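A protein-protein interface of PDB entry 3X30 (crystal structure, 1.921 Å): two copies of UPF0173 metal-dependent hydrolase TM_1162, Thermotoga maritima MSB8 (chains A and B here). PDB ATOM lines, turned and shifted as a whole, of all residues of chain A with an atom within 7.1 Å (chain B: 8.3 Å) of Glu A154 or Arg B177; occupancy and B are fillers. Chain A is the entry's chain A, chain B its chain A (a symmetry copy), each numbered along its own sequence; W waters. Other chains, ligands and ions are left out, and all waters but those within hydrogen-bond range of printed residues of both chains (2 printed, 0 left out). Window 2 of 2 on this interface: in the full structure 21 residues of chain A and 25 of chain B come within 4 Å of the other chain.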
ATOM      1  N   LYS A 103     -22.483 -26.975  17.193  1.00  0.00           N
ATOM      2  CA  LYS A 103     -22.535 -27.042  18.648  1.00  0.00           C
ATOM      3  C   LYS A 103     -23.483 -25.970  19.150  1.00  0.00           C
ATOM      4  O   LYS A 103     -23.416 -24.824  18.689  1.00  0.00           O
ATOM      5  CB  LYS A 103     -21.143 -26.838  19.248  1.00  0.00           C
ATOM      6  CG  LYS A 103     -21.100 -26.848  20.772  1.00  0.00           C
ATOM      7  CD  LYS A 103     -19.668 -26.613  21.235  1.00  0.00           C
ATOM      8  CE  LYS A 103     -19.476 -26.964  22.691  1.00  0.00           C
ATOM      9  NZ  LYS A 103     -18.012 -26.929  23.042  1.00  0.00           N
ATOM     10  N   LYS A 136     -14.871 -21.311  11.485  1.00  0.00           N
ATOM     11  CA  LYS A 136     -15.837 -21.294  12.584  1.00  0.00           C
ATOM     12  C   LYS A 136     -16.688 -20.032  12.605  1.00  0.00           C
ATOM     13  O   LYS A 136     -16.167 -18.914  12.617  1.00  0.00           O
ATOM     14  CB  LYS A 136     -15.116 -21.466  13.924  1.00  0.00           C
ATOM     15  CG  LYS A 136     -14.476 -22.837  14.083  1.00  0.00           C
ATOM     16  CD  LYS A 136     -13.751 -22.964  15.407  1.00  0.00           C
ATOM     17  CE  LYS A 136     -12.993 -24.280  15.513  1.00  0.00           C
ATOM     18  NZ  LYS A 136     -12.119 -24.254  16.715  1.00  0.00           N
ATOM     19  N   MET A 149     -19.386 -17.220  27.424  1.00  0.00           N
ATOM     20  CA  MET A 149     -18.747 -16.802  26.178  1.00  0.00           C
ATOM     21  C   MET A 149     -17.225 -16.954  26.218  1.00  0.00           C
ATOM     22  O   MET A 149     -16.586 -17.136  25.189  1.00  0.00           O
ATOM     23  CB  MET A 149     -19.117 -15.356  25.858  1.00  0.00           C
ATOM     24  CG  MET A 149     -20.566 -15.215  25.452  1.00  0.00           C
ATOM     25  SD  MET A 149     -21.142 -13.362  25.628  1.00  0.00           S
ATOM     26  CE  MET A 149     -22.890 -13.564  24.754  1.00  0.00           C
ATOM     27  N   GLU A 150     -16.649 -16.900  27.412  1.00  0.00           N
ATOM     28  CA  GLU A 150     -15.199 -17.045  27.549  1.00  0.00           C
ATOM     29  C   GLU A 150     -14.740 -18.452  27.139  1.00  0.00           C
ATOM     30  O   GLU A 150     -13.569 -18.659  26.811  1.00  0.00           O
ATOM     31  CB  GLU A 150     -14.769 -16.724  28.988  1.00  0.00           C
ATOM     32  CG  GLU A 150     -14.867 -15.238  29.315  1.00  0.00           C
ATOM     33  CD  GLU A 150     -14.797 -14.935  30.805  1.00  0.00           C
ATOM     34  OE1 GLU A 150     -15.255 -15.766  31.622  1.00  0.00           O
ATOM     35  OE2 GLU A 150     -14.280 -13.853  31.151  1.00  0.00           O
ATOM     36  N   LEU A 151     -15.665 -19.412  27.130  1.00  0.00           N
ATOM     37  CA  LEU A 151     -15.342 -20.782  26.700  1.00  0.00           C
ATOM     38  C   LEU A 151     -15.011 -20.833  25.212  1.00  0.00           C
ATOM     39  O   LEU A 151     -14.437 -21.814  24.733  1.00  0.00           O
ATOM     40  CB  LEU A 151     -16.505 -21.748  26.994  1.00  0.00           C
ATOM     41  CG  LEU A 151     -16.896 -21.916  28.465  1.00  0.00           C
ATOM     42  CD1 LEU A 151     -18.117 -22.819  28.597  1.00  0.00           C
ATOM     43  CD2 LEU A 151     -15.731 -22.467  29.258  1.00  0.00           C
ATOM     44  N   LEU A 152     -15.384 -19.782  24.486  1.00  0.00           N
ATOM     45  CA  LEU A 152     -15.229 -19.741  23.033  1.00  0.00           C
ATOM     46  C   LEU A 152     -13.893 -19.145  22.586  1.00  0.00           C
ATOM     47  O   LEU A 152     -13.522 -19.255  21.416  1.00  0.00           O
ATOM     48  CB  LEU A 152     -16.369 -18.932  22.413  1.00  0.00           C
ATOM     49  CG  LEU A 152     -17.782 -19.481  22.666  1.00  0.00           C
ATOM     50  CD1 LEU A 152     -18.827 -18.513  22.137  1.00  0.00           C
ATOM     51  CD2 LEU A 152     -17.937 -20.853  22.013  1.00  0.00           C
ATOM     52  N   ALA A 153     -13.194 -18.489  23.503  1.00  0.00           N
ATOM     53  CA  ALA A 153     -11.938 -17.841  23.139  1.00  0.00           C
ATOM     54  C   ALA A 153     -10.973 -18.850  22.517  1.00  0.00           C
ATOM     55  O   ALA A 153     -10.371 -18.582  21.473  1.00  0.00           O
ATOM     56  CB  ALA A 153     -11.314 -17.160  24.353  1.00  0.00           C
ATOM     57  N   GLU A 154     -10.860 -20.030  23.116  1.00  0.00           N
ATOM     58  CA  GLU A 154      -9.899 -21.016  22.613  1.00  0.00           C
ATOM     59  C   GLU A 154     -10.286 -21.604  21.254  1.00  0.00           C
ATOM     60  O   GLU A 154      -9.480 -22.289  20.627  1.00  0.00           O
ATOM     61  CB  GLU A 154      -9.711 -22.143  23.628  1.00  0.00           C
ATOM     62  CG  GLU A 154     -10.885 -23.102  23.745  1.00  0.00           C
ATOM     63  CD  GLU A 154     -10.541 -24.308  24.611  1.00  0.00           C
ATOM     64  OE1 GLU A 154     -10.108 -24.106  25.763  1.00  0.00           O
ATOM     65  OE2 GLU A 154     -10.679 -25.453  24.130  1.00  0.00           O
ATOM     66  N   GLU A 155     -11.507 -21.339  20.790  1.00  0.00           N
ATOM     67  CA  GLU A 155     -11.938 -21.837  19.486  1.00  0.00           C
ATOM     68  C   GLU A 155     -11.327 -21.051  18.316  1.00  0.00           C
ATOM     69  O   GLU A 155     -11.279 -21.560  17.192  1.00  0.00           O
ATOM     70  CB  GLU A 155     -13.466 -21.801  19.376  1.00  0.00           C
ATOM     71  CG  GLU A 155     -14.185 -22.639  20.436  1.00  0.00           C
ATOM     72  CD  GLU A 155     -14.136 -24.126  20.147  1.00  0.00           C
ATOM     73  OE1 GLU A 155     -13.840 -24.509  18.990  1.00  0.00           O
ATOM     74  OE2 GLU A 155     -14.411 -24.915  21.080  1.00  0.00           O
ATOM     75  N   ASN A 156     -10.882 -19.821  18.584  1.00  0.00           N
ATOM     76  CA  ASN A 156     -10.401 -18.902  17.543  1.00  0.00           C
ATOM     77  C   ASN A 156     -11.454 -18.754  16.444  1.00  0.00           C
ATOM     78  O   ASN A 156     -11.204 -19.014  15.263  1.00  0.00           O
ATOM     79  CB  ASN A 156      -9.056 -19.384  16.966  1.00  0.00           C
ATOM     80  CG  ASN A 156      -8.280 -18.274  16.253  1.00  0.00           C
ATOM     81  OD1 ASN A 156      -8.698 -17.115  16.226  1.00  0.00           O
ATOM     82  ND2 ASN A 156      -7.128 -18.633  15.682  1.00  0.00           N
ATOM     83  N   VAL A 157     -12.650 -18.344  16.862  1.00  0.00           N
ATOM     84  CA  VAL A 157     -13.783 -18.105  15.973  1.00  0.00           C
ATOM     85  C   VAL A 157     -13.421 -17.147  14.824  1.00  0.00           C
ATOM     86  O   VAL A 157     -12.807 -16.112  15.054  1.00  0.00           O
ATOM     87  CB  VAL A 157     -14.976 -17.525  16.788  1.00  0.00           C
ATOM     88  CG1 VAL A 157     -16.069 -16.997  15.875  1.00  0.00           C
ATOM     89  CG2 VAL A 157     -15.523 -18.583  17.754  1.00  0.00           C
ATOM     90  N   MET A 181     -14.246 -10.934  25.359  1.00  0.00           N
ATOM     91  CA  MET A 181     -14.270 -12.283  25.919  1.00  0.00           C
ATOM     92  C   MET A 181     -14.015 -13.372  24.876  1.00  0.00           C
ATOM     93  O   MET A 181     -13.305 -14.347  25.127  1.00  0.00           O
ATOM     94  CB  MET A 181     -15.626 -12.566  26.570  1.00  0.00           C
ATOM     95  CG  MET A 181     -15.859 -11.973  27.928  1.00  0.00           C
ATOM     96  SD  MET A 181     -17.645 -12.635  28.448  1.00  0.00           S
ATOM     97  CE  MET A 181     -17.682 -11.938  30.265  1.00  0.00           C
ATOM     98  N   ILE A 182     -14.627 -13.215  23.714  1.00  0.00           N
ATOM     99  CA  ILE A 182     -14.629 -14.269  22.700  1.00  0.00           C
ATOM    100  C   ILE A 182     -13.385 -14.202  21.815  1.00  0.00           C
ATOM    101  O   ILE A 182     -12.884 -15.229  21.346  1.00  0.00           O
ATOM    102  CB  ILE A 182     -15.901 -14.179  21.820  1.00  0.00           C
ATOM    103  CG1 ILE A 182     -17.148 -14.396  22.679  1.00  0.00           C
ATOM    104  CG2 ILE A 182     -15.875 -15.215  20.701  1.00  0.00           C
ATOM    105  CD1 ILE A 182     -18.449 -13.964  22.001  1.00  0.00           C
ATOM    106  N   LEU B 145     -20.852 -27.927  28.853  1.00  0.00           N
ATOM    107  CA  LEU B 145     -19.772 -27.308  29.596  1.00  0.00           C
ATOM    108  C   LEU B 145     -20.218 -25.927  30.090  1.00  0.00           C
ATOM    109  O   LEU B 145     -20.761 -25.144  29.321  1.00  0.00           O
ATOM    110  CB  LEU B 145     -18.535 -27.197  28.708  1.00  0.00           C
ATOM    111  CG  LEU B 145     -17.278 -26.652  29.385  1.00  0.00           C
ATOM    112  CD1 LEU B 145     -16.853 -27.600  30.494  1.00  0.00           C
ATOM    113  CD2 LEU B 145     -16.182 -26.498  28.333  1.00  0.00           C
ATOM    114  N   THR B 146     -20.003 -25.641  31.369  1.00  0.00           N
ATOM    115  CA  THR B 146     -20.356 -24.337  31.915  1.00  0.00           C
ATOM    116  C   THR B 146     -19.329 -23.903  32.963  1.00  0.00           C
ATOM    117  O   THR B 146     -18.814 -24.724  33.732  1.00  0.00           O
ATOM    118  CB  THR B 146     -21.771 -24.345  32.543  1.00  0.00           C
ATOM    119  OG1 THR B 146     -21.933 -23.180  33.354  1.00  0.00           O
ATOM    120  CG2 THR B 146     -21.975 -25.579  33.413  1.00  0.00           C
ATOM    121  N   ARG B 147     -19.037 -22.609  33.010  1.00  0.00           N
ATOM    122  CA  ARG B 147     -18.059 -22.122  33.980  1.00  0.00           C
ATOM    123  C   ARG B 147     -18.575 -22.274  35.418  1.00  0.00           C
ATOM    124  O   ARG B 147     -17.804 -22.152  36.374  1.00  0.00           O
ATOM    125  CB  ARG B 147     -17.686 -20.668  33.686  1.00  0.00           C
ATOM    126  CG  ARG B 147     -17.069 -20.467  32.304  1.00  0.00           C
ATOM    127  CD  ARG B 147     -16.077 -19.322  32.290  1.00  0.00           C
ATOM    128  NE  ARG B 147     -14.899 -19.637  33.094  1.00  0.00           N
ATOM    129  CZ  ARG B 147     -13.793 -18.902  33.133  1.00  0.00           C
ATOM    130  NH1 ARG B 147     -13.701 -17.792  32.411  1.00  0.00           N
ATOM    131  NH2 ARG B 147     -12.774 -19.282  33.899  1.00  0.00           N
ATOM    132  N   MET B 149     -19.280 -24.886  36.787  1.00  0.00           N
ATOM    133  CA  MET B 149     -18.589 -26.058  37.318  1.00  0.00           C
ATOM    134  C   MET B 149     -17.328 -25.691  38.105  1.00  0.00           C
ATOM    135  O   MET B 149     -16.914 -26.418  38.999  1.00  0.00           O
ATOM    136  CB  MET B 149     -18.234 -27.018  36.185  1.00  0.00           C
ATOM    137  CG  MET B 149     -19.456 -27.692  35.608  1.00  0.00           C
ATOM    138  SD  MET B 149     -19.059 -28.419  33.844  1.00  0.00           S
ATOM    139  CE  MET B 149     -20.734 -29.418  33.606  1.00  0.00           C
ATOM    140  N   GLU B 150     -16.732 -24.550  37.782  1.00  0.00           N
ATOM    141  CA  GLU B 150     -15.526 -24.113  38.486  1.00  0.00           C
ATOM    142  C   GLU B 150     -15.824 -23.803  39.960  1.00  0.00           C
ATOM    143  O   GLU B 150     -14.918 -23.803  40.796  1.00  0.00           O
ATOM    144  CB  GLU B 150     -14.916 -22.892  37.781  1.00  0.00           C
ATOM    145  CG  GLU B 150     -14.268 -23.244  36.446  1.00  0.00           C
ATOM    146  CD  GLU B 150     -13.979 -22.036  35.569  1.00  0.00           C
ATOM    147  OE1 GLU B 150     -14.735 -21.039  35.631  1.00  0.00           O
ATOM    148  OE2 GLU B 150     -12.987 -22.093  34.814  1.00  0.00           O
ATOM    149  N   LEU B 162     -20.085 -37.512  35.122  1.00  0.00           N
ATOM    150  CA  LEU B 162     -20.158 -36.527  34.044  1.00  0.00           C
ATOM    151  C   LEU B 162     -20.678 -37.169  32.763  1.00  0.00           C
ATOM    152  O   LEU B 162     -20.213 -38.243  32.374  1.00  0.00           O
ATOM    153  CB  LEU B 162     -18.780 -35.908  33.762  1.00  0.00           C
ATOM    154  CG  LEU B 162     -18.018 -35.154  34.853  1.00  0.00           C
ATOM    155  CD1 LEU B 162     -16.735 -34.622  34.257  1.00  0.00           C
ATOM    156  CD2 LEU B 162     -18.842 -34.010  35.437  1.00  0.00           C
ATOM    157  N   MET B 170     -22.484 -32.807  26.944  1.00  0.00           N
ATOM    158  CA  MET B 170     -21.061 -32.720  26.621  1.00  0.00           C
ATOM    159  C   MET B 170     -20.575 -33.950  25.871  1.00  0.00           C
ATOM    160  O   MET B 170     -20.999 -35.064  26.174  1.00  0.00           O
ATOM    161  CB  MET B 170     -20.227 -32.572  27.897  1.00  0.00           C
ATOM    162  CG  MET B 170     -20.537 -31.338  28.708  1.00  0.00           C
ATOM    163  SD  MET B 170     -19.197 -31.120  30.113  1.00  0.00           S
ATOM    164  CE  MET B 170     -19.758 -32.590  31.266  1.00  0.00           C
ATOM    165  N   ASP B 171     -19.694 -33.750  24.897  1.00  0.00           N
ATOM    166  CA  ASP B 171     -18.998 -34.879  24.286  1.00  0.00           C
ATOM    167  C   ASP B 171     -17.720 -35.148  25.082  1.00  0.00           C
ATOM    168  O   ASP B 171     -17.508 -34.562  26.151  1.00  0.00           O
ATOM    169  CB  ASP B 171     -18.694 -34.625  22.798  1.00  0.00           C
ATOM    170  CG  ASP B 171     -17.790 -33.416  22.562  1.00  0.00           C
ATOM    171  OD1 ASP B 171     -17.328 -32.772  23.527  1.00  0.00           O
ATOM    172  OD2 ASP B 171     -17.533 -33.100  21.381  1.00  0.00           O
ATOM    173  N   VAL B 172     -16.873 -36.033  24.575  1.00  0.00           N
ATOM    174  CA  VAL B 172     -15.699 -36.456  25.328  1.00  0.00           C
ATOM    175  C   VAL B 172     -14.770 -35.280  25.592  1.00  0.00           C
ATOM    176  O   VAL B 172     -14.274 -35.101  26.706  1.00  0.00           O
ATOM    177  CB  VAL B 172     -14.939 -37.576  24.590  1.00  0.00           C
ATOM    178  CG1 VAL B 172     -13.514 -37.699  25.119  1.00  0.00           C
ATOM    179  CG2 VAL B 172     -15.696 -38.898  24.727  1.00  0.00           C
ATOM    180  N   GLU B 173     -14.554 -34.461  24.573  1.00  0.00           N
ATOM    181  CA  GLU B 173     -13.598 -33.361  24.679  1.00  0.00           C
ATOM    182  C   GLU B 173     -14.046 -32.325  25.706  1.00  0.00           C
ATOM    183  O   GLU B 173     -13.241 -31.845  26.508  1.00  0.00           O
ATOM    184  CB  GLU B 173     -13.392 -32.699  23.314  1.00  0.00           C
ATOM    185  CG  GLU B 173     -12.633 -33.568  22.292  1.00  0.00           C
ATOM    186  CD  GLU B 173     -13.340 -34.879  21.938  1.00  0.00           C
ATOM    187  OE1 GLU B 173     -14.592 -34.888  21.773  1.00  0.00           O
ATOM    188  OE2 GLU B 173     -12.636 -35.914  21.834  1.00  0.00           O
ATOM    189  N   ASP B 174     -15.328 -31.969  25.683  1.00  0.00           N
ATOM    190  CA  ASP B 174     -15.809 -30.980  26.633  1.00  0.00           C
ATOM    191  C   ASP B 174     -15.888 -31.571  28.035  1.00  0.00           C
ATOM    192  O   ASP B 174     -15.680 -30.850  29.007  1.00  0.00           O
ATOM    193  CB  ASP B 174     -17.166 -30.411  26.191  1.00  0.00           C
ATOM    194  CG  ASP B 174     -17.011 -29.184  25.284  1.00  0.00           C
ATOM    195  OD1 ASP B 174     -15.872 -28.907  24.845  1.00  0.00           O
ATOM    196  OD2 ASP B 174     -18.014 -28.480  25.024  1.00  0.00           O
ATOM    197  N   ALA B 175     -16.157 -32.873  28.155  1.00  0.00           N
ATOM    198  CA  ALA B 175     -16.202 -33.482  29.483  1.00  0.00           C
ATOM    199  C   ALA B 175     -14.808 -33.521  30.122  1.00  0.00           C
ATOM    200  O   ALA B 175     -14.682 -33.454  31.342  1.00  0.00           O
ATOM    201  CB  ALA B 175     -16.788 -34.878  29.429  1.00  0.00           C
ATOM    202  N   VAL B 176     -13.770 -33.658  29.300  1.00  0.00           N
ATOM    203  CA  VAL B 176     -12.404 -33.544  29.802  1.00  0.00           C
ATOM    204  C   VAL B 176     -12.175 -32.135  30.361  1.00  0.00           C
ATOM    205  O   VAL B 176     -11.645 -31.967  31.466  1.00  0.00           O
ATOM    206  CB  VAL B 176     -11.365 -33.872  28.699  1.00  0.00           C
ATOM    207  CG1 VAL B 176      -9.950 -33.531  29.164  1.00  0.00           C
ATOM    208  CG2 VAL B 176     -11.469 -35.343  28.304  1.00  0.00           C
ATOM    209  N   ARG B 177     -12.579 -31.116  29.610  1.00  0.00           N
ATOM    210  CA  ARG B 177     -12.500 -29.750  30.116  1.00  0.00           C
ATOM    211  C   ARG B 177     -13.253 -29.583  31.437  1.00  0.00           C
ATOM    212  O   ARG B 177     -12.773 -28.892  32.342  1.00  0.00           O
ATOM    213  CB  ARG B 177     -13.029 -28.751  29.086  1.00  0.00           C
ATOM    214  CG  ARG B 177     -12.165 -28.643  27.840  1.00  0.00           C
ATOM    215  CD  ARG B 177     -12.883 -27.880  26.749  1.00  0.00           C
ATOM    216  NE  ARG B 177     -12.924 -26.445  27.003  1.00  0.00           N
ATOM    217  CZ  ARG B 177     -13.596 -25.580  26.248  1.00  0.00           C
ATOM    218  NH1 ARG B 177     -14.304 -26.015  25.213  1.00  0.00           N
ATOM    219  NH2 ARG B 177     -13.577 -24.285  26.533  1.00  0.00           N
ATOM    220  N   ALA B 178     -14.428 -30.205  31.544  1.00  0.00           N
ATOM    221  CA  ALA B 178     -15.209 -30.143  32.780  1.00  0.00           C
ATOM    222  C   ALA B 178     -14.469 -30.776  33.961  1.00  0.00           C
ATOM    223  O   ALA B 178     -14.457 -30.231  35.071  1.00  0.00           O
ATOM    224  CB  ALA B 178     -16.565 -30.831  32.585  1.00  0.00           C
ATOM    225  N   ALA B 179     -13.884 -31.944  33.726  1.00  0.00           N
ATOM    226  CA  ALA B 179     -13.108 -32.642  34.757  1.00  0.00           C
ATOM    227  C   ALA B 179     -11.953 -31.787  35.277  1.00  0.00           C
ATOM    228  O   ALA B 179     -11.667 -31.774  36.474  1.00  0.00           O
ATOM    229  CB  ALA B 179     -12.577 -33.958  34.207  1.00  0.00           C
ATOM    230  N   VAL B 180     -11.298 -31.079  34.367  1.00  0.00           N
ATOM    231  CA  VAL B 180     -10.199 -30.178  34.716  1.00  0.00           C
ATOM    232  C   VAL B 180     -10.689 -28.983  35.550  1.00  0.00           C
ATOM    233  O   VAL B 180     -10.016 -28.543  36.490  1.00  0.00           O
ATOM    234  CB  VAL B 180      -9.494 -29.679  33.439  1.00  0.00           C
ATOM    235  CG1 VAL B 180      -8.492 -28.570  33.752  1.00  0.00           C
ATOM    236  CG2 VAL B 180      -8.812 -30.845  32.732  1.00  0.00           C
ATOM    237  N   MET B 181     -11.872 -28.469  35.211  1.00  0.00           N
ATOM    238  CA  MET B 181     -12.512 -27.408  35.984  1.00  0.00           C
ATOM    239  C   MET B 181     -12.870 -27.832  37.408  1.00  0.00           C
ATOM    240  O   MET B 181     -12.705 -27.072  38.365  1.00  0.00           O
ATOM    241  CB  MET B 181     -13.798 -26.947  35.294  1.00  0.00           C
ATOM    242  CG  MET B 181     -13.642 -26.030  34.118  1.00  0.00           C
ATOM    243  SD  MET B 181     -15.494 -25.602  33.584  1.00  0.00           S
ATOM    244  CE  MET B 181     -15.091 -24.285  32.208  1.00  0.00           C
ATOM    245  N   ILE B 182     -13.394 -29.040  37.538  1.00  0.00           N
ATOM    246  CA  ILE B 182     -13.959 -29.497  38.807  1.00  0.00           C
ATOM    247  C   ILE B 182     -12.887 -30.093  39.718  1.00  0.00           C
ATOM    248  O   ILE B 182     -12.969 -29.990  40.946  1.00  0.00           O
ATOM    249  CB  ILE B 182     -15.077 -30.541  38.563  1.00  0.00           C
ATOM    250  CG1 ILE B 182     -16.226 -29.904  37.777  1.00  0.00           C
ATOM    251  CG2 ILE B 182     -15.615 -31.094  39.879  1.00  0.00           C
ATOM    252  CD1 ILE B 182     -17.193 -30.917  37.165  1.00  0.00           C
ATOM    253  N   LYS B 183     -11.886 -30.709  39.099  1.00  0.00           N
ATOM    254  CA  LYS B 183     -10.816 -31.436  39.808  1.00  0.00           C
ATOM    255  C   LYS B 183     -11.307 -32.372  40.913  1.00  0.00           C
ATOM    256  O   LYS B 183     -10.898 -32.235  42.068  1.00  0.00           O
ATOM    257  CB  LYS B 183      -9.811 -30.447  40.403  1.00  0.00           C
ATOM    258  CG  LYS B 183      -9.231 -29.495  39.387  1.00  0.00           C
ATOM    259  CD  LYS B 183      -7.955 -28.838  39.892  1.00  0.00           C
ATOM    260  CE  LYS B 183      -7.518 -27.747  38.938  1.00  0.00           C
ATOM    261  NZ  LYS B 183      -8.514 -26.642  38.917  1.00  0.00           N
ATOM    262  N   PHE B 205     -12.014 -41.191  26.565  1.00  0.00           N
ATOM    263  CA  PHE B 205     -12.269 -40.270  27.664  1.00  0.00           C
ATOM    264  C   PHE B 205     -11.368 -40.600  28.857  1.00  0.00           C
ATOM    265  O   PHE B 205     -10.708 -39.707  29.420  1.00  0.00           O
ATOM    266  CB  PHE B 205     -13.743 -40.304  28.094  1.00  0.00           C
ATOM    267  CG  PHE B 205     -14.016 -39.470  29.319  1.00  0.00           C
ATOM    268  CD1 PHE B 205     -14.081 -38.087  29.224  1.00  0.00           C
ATOM    269  CD2 PHE B 205     -14.169 -40.064  30.562  1.00  0.00           C
ATOM    270  CE1 PHE B 205     -14.316 -37.304  30.362  1.00  0.00           C
ATOM    271  CE2 PHE B 205     -14.406 -39.291  31.702  1.00  0.00           C
ATOM    272  CZ  PHE B 205     -14.481 -37.907  31.595  1.00  0.00           C
ATOM    273  N   LYS B 208      -7.755 -39.613  28.087  1.00  0.00           N
ATOM    274  CA  LYS B 208      -7.504 -38.173  28.054  1.00  0.00           C
ATOM    275  C   LYS B 208      -7.650 -37.478  29.411  1.00  0.00           C
ATOM    276  O   LYS B 208      -6.916 -36.535  29.718  1.00  0.00           O
ATOM    277  CB  LYS B 208      -8.426 -37.505  27.042  1.00  0.00           C
ATOM    278  CG  LYS B 208      -8.143 -37.906  25.600  1.00  0.00           C
ATOM    279  CD  LYS B 208      -9.023 -37.115  24.649  1.00  0.00           C
ATOM    280  CE  LYS B 208      -8.604 -37.333  23.201  1.00  0.00           C
ATOM    281  NZ  LYS B 208      -9.187 -36.295  22.307  1.00  0.00           N
ATOM    282  N   VAL B 209      -8.607 -37.911  30.223  1.00  0.00           N
ATOM    283  CA  VAL B 209      -8.796 -37.218  31.486  1.00  0.00           C
ATOM    284  C   VAL B 209      -7.676 -37.619  32.458  1.00  0.00           C
ATOM    285  O   VAL B 209      -7.222 -36.807  33.265  1.00  0.00           O
ATOM    286  CB  VAL B 209     -10.201 -37.481  32.085  1.00  0.00           C
ATOM    287  CG1 VAL B 209     -10.314 -38.867  32.620  1.00  0.00           C
ATOM    288  CG2 VAL B 209     -10.482 -36.490  33.181  1.00  0.00           C
ATOM    289  N   LYS B 212      -4.688 -35.562  32.122  1.00  0.00           N
ATOM    290  CA  LYS B 212      -4.807 -34.253  32.758  1.00  0.00           C
ATOM    291  C   LYS B 212      -4.683 -34.369  34.276  1.00  0.00           C
ATOM    292  O   LYS B 212      -4.773 -33.371  34.989  1.00  0.00           O
ATOM    293  CB  LYS B 212      -6.140 -33.582  32.391  1.00  0.00           C
ATOM    294  CG  LYS B 212      -6.297 -33.267  30.917  1.00  0.00           C
ATOM    295  CD  LYS B 212      -5.195 -32.342  30.430  1.00  0.00           C
ATOM    296  CE  LYS B 212      -5.433 -31.917  28.985  1.00  0.00           C
ATOM    297  NZ  LYS B 212      -4.203 -31.316  28.381  1.00  0.00           N
HETATM  298  O   HOH W   1     -11.331 -22.658  27.343  1.00  0.00           O
HETATM  299  O   HOH W   2     -15.229 -24.035  23.295  1.00  0.00           O
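The side-chain carboxylate of Asp B174 is in salt-bridge range of the side-chain amino group of Lys A103 (2.5 Å). OE1 of Glu A150 is in salt-bridge range of NH1 of Arg B147, at 2.7 Å. The backbone carbonyl oxygen of Leu A151 is in hydrogen-bond range of the guanidinium group of Arg B177, 3.2 Å away. The side-chain carboxylate (OE1) of Glu A154 is in salt-bridge range of the guanidinium group (NH2) of Arg B177, 3.6 Å away.
NE of Arg B147 is in salt-bridge range of OE1 of Glu B150 (2.9 Å). The side-chain carboxylate (OD1) of Asp B171 lies within hydrogen-bond range of the backbone NH (N) of Asp B174, 3.0 Å away. NH1 of Arg B177 is in salt-bridge range of OD1 of Asp B174 (3.3 Å).
Leu A151 touches Leu B145. Leu A151 touches Arg B147 (CD2 to CG, 3.9 Å). CE of Met B181 touches CD2 of Leu A151 (3.5 Å).
Of the printed residues of chain B, Leu A151 touches Leu B145 (3.6 Å), Arg B147 (3.9 Å), Arg B177 (3.2 Å) and Met B181 (3.5 Å). Glu A154 touches just one residue of chain B: Arg B177. Asp B171 touches none of the printed residues of chain A. Arg B177 touches two residues of chain A. Val B180 touches none of the printed residues of chain A. Of the printed residues of chain A, Met B181 touches Leu A151 (3.5 Å).
Of the 24 printed residues of chain B, 5 touch a printed residue of chain A. Hydrophobic or aromatic side chains of chain B within 4 Å of the printed part of chain A: Met B181. Of the 13 printed residues of chain A, 4 touch a printed residue of chain B. Printed residues of chain A that touch a printed residue of chain B: Lys A103, Glu A150, Leu A151 and Glu A154. Hydrophobic or aromatic side chains of chain A that line the printed part of chain B: Leu A151. Along chain A the printed residues that touch a printed residue of chain B span positions 103 to 154.
Positions printed for both chains: 149, 150, 181 and 182. Of the 7 pairs that touch across the chains among the printed residues, none has its exchanged pair printed and touching as well.
Water W1 lies within hydrogen-bond range of the side-chain carboxylate of Glu A154 (2.5 Å) and the guanidinium group of Arg B177 (2.9 Å). Water W2 lies within hydrogen-bond range of the side-chain carboxylate (OE2) of Glu A155, the backbone carbonyl oxygen (O) of Leu A151 and the guanidinium group (NH1) of Arg B177.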
